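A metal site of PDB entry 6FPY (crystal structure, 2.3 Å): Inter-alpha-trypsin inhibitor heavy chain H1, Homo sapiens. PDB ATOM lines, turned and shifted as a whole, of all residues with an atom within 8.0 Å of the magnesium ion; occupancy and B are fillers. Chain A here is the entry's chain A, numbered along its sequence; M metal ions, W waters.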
ATOM      1  N   ASP A 286      12.613  13.143  26.663  1.00  0.00           N
ATOM      2  CA  ASP A 286      12.674  11.899  25.907  1.00  0.00           C
ATOM      3  C   ASP A 286      12.397  12.176  24.431  1.00  0.00           C
ATOM      4  O   ASP A 286      11.397  12.803  24.089  1.00  0.00           O
ATOM      5  CB  ASP A 286      11.655  10.912  26.465  1.00  0.00           C
ATOM      6  CG  ASP A 286      11.771   9.526  25.859  1.00  0.00           C
ATOM      7  OD1 ASP A 286      12.541   9.342  24.894  1.00  0.00           O
ATOM      8  OD2 ASP A 286      11.093   8.610  26.369  1.00  0.00           O
ATOM      9  N   ILE A 287      13.299  11.715  23.562  1.00  0.00           N
ATOM     10  CA  ILE A 287      13.086  11.855  22.116  1.00  0.00           C
ATOM     11  C   ILE A 287      13.133  10.485  21.446  1.00  0.00           C
ATOM     12  O   ILE A 287      13.682  10.341  20.344  1.00  0.00           O
ATOM     13  CB  ILE A 287      14.123  12.817  21.505  1.00  0.00           C
ATOM     14  CG1 ILE A 287      15.549  12.281  21.681  1.00  0.00           C
ATOM     15  CG2 ILE A 287      13.985  14.191  22.130  1.00  0.00           C
ATOM     16  CD1 ILE A 287      16.570  12.972  20.789  1.00  0.00           C
ATOM     17  N   SER A 288      12.548   9.488  22.092  1.00  0.00           N
ATOM     18  CA  SER A 288      12.476   8.148  21.534  1.00  0.00           C
ATOM     19  C   SER A 288      11.468   8.119  20.395  1.00  0.00           C
ATOM     20  O   SER A 288      10.592   8.988  20.272  1.00  0.00           O
ATOM     21  CB  SER A 288      12.103   7.129  22.607  1.00  0.00           C
ATOM     22  OG  SER A 288      10.765   7.311  23.042  1.00  0.00           O
ATOM     23  N   GLY A 289      11.571   7.088  19.548  1.00  0.00           N
ATOM     24  CA  GLY A 289      10.649   6.978  18.431  1.00  0.00           C
ATOM     25  C   GLY A 289       9.196   6.943  18.841  1.00  0.00           C
ATOM     26  O   GLY A 289       8.326   7.407  18.097  1.00  0.00           O
ATOM     27  N   SER A 290       8.898   6.389  20.029  1.00  0.00           N
ATOM     28  CA  SER A 290       7.510   6.324  20.483  1.00  0.00           C
ATOM     29  C   SER A 290       6.894   7.705  20.629  1.00  0.00           C
ATOM     30  O   SER A 290       5.672   7.833  20.558  1.00  0.00           O
ATOM     31  CB  SER A 290       7.429   5.574  21.807  1.00  0.00           C
ATOM     32  OG  SER A 290       8.241   6.172  22.809  1.00  0.00           O
ATOM     33  N   MET A 291       7.725   8.747  20.802  1.00  0.00           N
ATOM     34  CA  MET A 291       7.254  10.126  20.915  1.00  0.00           C
ATOM     35  C   MET A 291       6.723  10.678  19.608  1.00  0.00           C
ATOM     36  O   MET A 291       6.168  11.783  19.602  1.00  0.00           O
ATOM     37  CB  MET A 291       8.401  11.005  21.418  1.00  0.00           C
ATOM     38  CG  MET A 291       8.841  10.742  22.851  1.00  0.00           C
ATOM     39  SD  MET A 291       7.678  11.351  24.089  1.00  0.00           S
ATOM     40  CE  MET A 291       7.784  13.109  23.820  1.00  0.00           C
ATOM     41  N   ARG A 292       6.871   9.945  18.515  1.00  0.00           N
ATOM     42  CA  ARG A 292       6.503  10.453  17.193  1.00  0.00           C
ATOM     43  C   ARG A 292       5.033  10.840  17.165  1.00  0.00           C
ATOM     44  O   ARG A 292       4.166  10.121  17.681  1.00  0.00           O
ATOM     45  CB  ARG A 292       6.779   9.371  16.149  1.00  0.00           C
ATOM     46  CG  ARG A 292       6.836   9.845  14.719  1.00  0.00           C
ATOM     47  CD  ARG A 292       7.416   8.749  13.835  1.00  0.00           C
ATOM     48  NE  ARG A 292       8.853   8.575  14.055  1.00  0.00           N
ATOM     49  CZ  ARG A 292       9.796   9.405  13.613  1.00  0.00           C
ATOM     50  NH1 ARG A 292       9.468  10.500  12.932  1.00  0.00           N
ATOM     51  NH2 ARG A 292      11.072   9.153  13.872  1.00  0.00           N
ATOM     52  N   LYS A 295       2.771  13.680  20.722  1.00  0.00           N
ATOM     53  CA  LYS A 295       3.525  13.826  21.965  1.00  0.00           C
ATOM     54  C   LYS A 295       4.687  14.788  21.787  1.00  0.00           C
ATOM     55  O   LYS A 295       4.826  15.753  22.555  1.00  0.00           O
ATOM     56  CB  LYS A 295       4.002  12.453  22.439  1.00  0.00           C
ATOM     57  CG  LYS A 295       2.912  11.636  23.132  1.00  0.00           C
ATOM     58  CD  LYS A 295       3.417  10.293  23.630  1.00  0.00           C
ATOM     59  CE  LYS A 295       3.396   9.243  22.522  1.00  0.00           C
ATOM     60  NZ  LYS A 295       4.116   8.003  22.915  1.00  0.00           N
ATOM     61  N   PHE A 321      17.214  12.954  25.255  1.00  0.00           N
ATOM     62  CA  PHE A 321      17.732  11.587  25.322  1.00  0.00           C
ATOM     63  C   PHE A 321      16.872  10.665  24.484  1.00  0.00           C
ATOM     64  O   PHE A 321      15.661  10.535  24.724  1.00  0.00           O
ATOM     65  CB  PHE A 321      17.824  11.091  26.781  1.00  0.00           C
ATOM     66  CG  PHE A 321      16.506  10.952  27.481  1.00  0.00           C
ATOM     67  CD1 PHE A 321      15.905  12.045  28.103  1.00  0.00           C
ATOM     68  CD2 PHE A 321      15.884   9.721  27.572  1.00  0.00           C
ATOM     69  CE1 PHE A 321      14.702  11.911  28.767  1.00  0.00           C
ATOM     70  CE2 PHE A 321      14.667   9.570  28.236  1.00  0.00           C
ATOM     71  CZ  PHE A 321      14.077  10.676  28.836  1.00  0.00           C
ATOM     72  N   GLU A 354      15.238   7.105  18.043  1.00  0.00           N
ATOM     73  CA  GLU A 354      15.020   5.671  18.265  1.00  0.00           C
ATOM     74  C   GLU A 354      14.860   5.320  19.755  1.00  0.00           C
ATOM     75  O   GLU A 354      13.766   5.484  20.307  1.00  0.00           O
ATOM     76  CB  GLU A 354      16.097   4.813  17.576  1.00  0.00           C
ATOM     77  CG  GLU A 354      17.503   5.375  17.438  1.00  0.00           C
ATOM     78  CD  GLU A 354      18.510   4.302  17.061  1.00  0.00           C
ATOM     79  OE1 GLU A 354      18.333   3.667  15.996  1.00  0.00           O
ATOM     80  OE2 GLU A 354      19.481   4.089  17.825  1.00  0.00           O
ATOM     81  N   ALA A 355      15.906   4.791  20.395  1.00  0.00           N
ATOM     82  CA  ALA A 355      15.777   4.131  21.687  1.00  0.00           C
ATOM     83  C   ALA A 355      15.656   5.167  22.813  1.00  0.00           C
ATOM     84  O   ALA A 355      15.375   6.348  22.578  1.00  0.00           O
ATOM     85  CB  ALA A 355      16.948   3.196  21.917  1.00  0.00           C
ATOM     86  N   THR A 356      15.833   4.726  24.067  1.00  0.00           N
ATOM     87  CA  THR A 356      15.604   5.569  25.241  1.00  0.00           C
ATOM     88  C   THR A 356      16.701   5.346  26.277  1.00  0.00           C
ATOM     89  O   THR A 356      16.633   4.406  27.075  1.00  0.00           O
ATOM     90  CB  THR A 356      14.238   5.269  25.860  1.00  0.00           C
ATOM     91  OG1 THR A 356      13.216   5.450  24.865  1.00  0.00           O
ATOM     92  CG2 THR A 356      13.962   6.178  27.042  1.00  0.00           C
ATOM     93  N   THR A 390       9.086  11.629  29.990  1.00  0.00           N
ATOM     94  CA  THR A 390       9.295  10.393  29.253  1.00  0.00           C
ATOM     95  C   THR A 390       7.964   9.717  29.009  1.00  0.00           C
ATOM     96  O   THR A 390       7.023   9.838  29.808  1.00  0.00           O
ATOM     97  CB  THR A 390      10.229   9.433  30.010  1.00  0.00           C
ATOM     98  OG1 THR A 390      10.531   8.306  29.198  1.00  0.00           O
ATOM     99  CG2 THR A 390       9.591   8.966  31.311  1.00  0.00           C
ATOM    100  N   ASP A 391       7.864   9.027  27.868  1.00  0.00           N
ATOM    101  CA  ASP A 391       6.698   8.232  27.498  1.00  0.00           C
ATOM    102  C   ASP A 391       6.962   6.729  27.511  1.00  0.00           C
ATOM    103  O   ASP A 391       6.066   5.953  27.159  1.00  0.00           O
ATOM    104  CB  ASP A 391       6.187   8.636  26.109  1.00  0.00           C
ATOM    105  CG  ASP A 391       7.116   8.196  25.001  1.00  0.00           C
ATOM    106  OD1 ASP A 391       8.338   8.073  25.258  1.00  0.00           O
ATOM    107  OD2 ASP A 391       6.634   7.982  23.867  1.00  0.00           O
ATOM    108  N   GLY A 392       8.157   6.295  27.914  1.00  0.00           N
ATOM    109  CA  GLY A 392       8.465   4.878  27.885  1.00  0.00           C
ATOM    110  C   GLY A 392       9.581   4.532  28.852  1.00  0.00           C
ATOM    111  O   GLY A 392      10.148   5.390  29.522  1.00  0.00           O
ATOM    112  N   ASP A 393       9.866   3.235  28.924  1.00  0.00           N
ATOM    113  CA  ASP A 393      10.876   2.728  29.842  1.00  0.00           C
ATOM    114  C   ASP A 393      12.251   2.758  29.195  1.00  0.00           C
ATOM    115  O   ASP A 393      12.380   2.824  27.976  1.00  0.00           O
ATOM    116  CB  ASP A 393      10.530   1.297  30.238  1.00  0.00           C
ATOM    117  CG  ASP A 393       9.204   1.188  30.970  1.00  0.00           C
ATOM    118  OD1 ASP A 393       8.807   2.145  31.652  1.00  0.00           O
ATOM    119  OD2 ASP A 393       8.547   0.123  30.846  1.00  0.00           O
ATOM    120  N   PRO A 394      13.311   2.692  30.017  1.00  0.00           N
ATOM    121  CA  PRO A 394      14.677   2.712  29.468  1.00  0.00           C
ATOM    122  C   PRO A 394      14.953   1.486  28.599  1.00  0.00           C
ATOM    123  O   PRO A 394      14.678   0.353  29.000  1.00  0.00           O
ATOM    124  CB  PRO A 394      15.565   2.751  30.715  1.00  0.00           C
ATOM    125  CG  PRO A 394      14.709   2.281  31.826  1.00  0.00           C
ATOM    126  CD  PRO A 394      13.314   2.714  31.481  1.00  0.00           C
ATOM    127  N   THR A 395      15.506   1.723  27.409  1.00  0.00           N
ATOM    128  CA  THR A 395      15.869   0.657  26.503  1.00  0.00           C
ATOM    129  C   THR A 395      17.313   0.745  26.031  1.00  0.00           C
ATOM    130  O   THR A 395      17.771  -0.169  25.326  1.00  0.00           O
ATOM    131  CB  THR A 395      14.962   0.667  25.269  1.00  0.00           C
ATOM    132  OG1 THR A 395      15.026   1.941  24.616  1.00  0.00           O
ATOM    133  CG2 THR A 395      13.526   0.384  25.668  1.00  0.00           C
ATOM    134  N   PHE A 423       4.384  10.711  30.377  1.00  0.00           N
ATOM    135  CA  PHE A 423       3.537  11.062  29.243  1.00  0.00           C
ATOM    136  C   PHE A 423       2.911   9.780  28.696  1.00  0.00           C
ATOM    137  O   PHE A 423       3.591   8.969  28.055  1.00  0.00           O
ATOM    138  CB  PHE A 423       4.363  11.778  28.172  1.00  0.00           C
ATOM    139  CG  PHE A 423       3.555  12.702  27.285  1.00  0.00           C
ATOM    140  CD1 PHE A 423       2.176  12.606  27.209  1.00  0.00           C
ATOM    141  CD2 PHE A 423       4.195  13.672  26.524  1.00  0.00           C
ATOM    142  CE1 PHE A 423       1.446  13.461  26.393  1.00  0.00           C
ATOM    143  CE2 PHE A 423       3.466  14.527  25.708  1.00  0.00           C
ATOM    144  CZ  PHE A 423       2.099  14.421  25.651  1.00  0.00           C
ATOM    145  N   ASN A 426       2.203   4.078  28.841  1.00  0.00           N
ATOM    146  CA  ASN A 426       3.228   3.069  28.606  1.00  0.00           C
ATOM    147  C   ASN A 426       4.464   3.291  29.466  1.00  0.00           C
ATOM    148  O   ASN A 426       5.499   2.657  29.226  1.00  0.00           O
ATOM    149  CB  ASN A 426       3.620   3.019  27.131  1.00  0.00           C
ATOM    150  CG  ASN A 426       2.590   2.296  26.283  1.00  0.00           C
ATOM    151  OD1 ASN A 426       2.322   1.113  26.492  1.00  0.00           O
ATOM    152  ND2 ASN A 426       2.021   3.007  25.314  1.00  0.00           N
ATOM    153  N   VAL A 427       4.381   4.168  30.464  1.00  0.00           N
ATOM    154  CA  VAL A 427       5.491   4.410  31.369  1.00  0.00           C
ATOM    155  C   VAL A 427       5.242   3.678  32.682  1.00  0.00           C
ATOM    156  O   VAL A 427       4.101   3.424  33.072  1.00  0.00           O
ATOM    157  CB  VAL A 427       5.683   5.918  31.657  1.00  0.00           C
ATOM    158  CG1 VAL A 427       6.014   6.681  30.399  1.00  0.00           C
ATOM    159  CG2 VAL A 427       4.441   6.508  32.319  1.00  0.00           C
HETATM  160 MG    MG M   1       9.556   6.137  24.446  1.00  0.00          MG
HETATM  161  O   HOH W   1      10.745   5.812  26.318  1.00  0.00           O
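Water W1 lies within hydrogen-bond range of OD2 of Asp 286 (2.8 Å), OG1 of Thr 356 (2.9 Å) and N of Gly 392 (3.1 Å).
The magnesium ion is bound by OG of Ser 290 (2.1 Å), OG of Ser 288 (2.2 Å), water W1 (2.2 Å) and OD1 of Asp 391 (2.4 Å).
The magnesium ion has four donor atoms within binding distance.
The backbone carbonyl oxygen of Gly 392 is in hydrogen-bond range of the side-chain hydroxyl of Thr 390 (3.0 Å).
The backbone NH of Ser 288 sits at hydrogen-bond distance from the side-chain carboxylate of Asp 286.
The backbone carbonyl oxygen (O) of Ser 290 is in hydrogen-bond range of the side-chain amino group (NZ) of Lys 295 (2.8 Å).
O of Thr 356 lies within hydrogen-bond range of N of Thr 395, at 2.9 Å.
OD2 of Asp 286 is in hydrogen-bond range of OG1 of Thr 390, at 2.9 Å.
OD2 of Asp 391 lies within salt-bridge range of NZ of Lys 295.
OD2 of Asp 391 sits at hydrogen-bond distance from N of Met 291.
Merely in contact with the magnesium ion: Asp 286 (3.5 Å), Thr 356 (3.7 Å) and Gly 392 (3.7 Å).
The nearest printed residue that does not touch the magnesium ion is Met 291 (4.8 Å).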
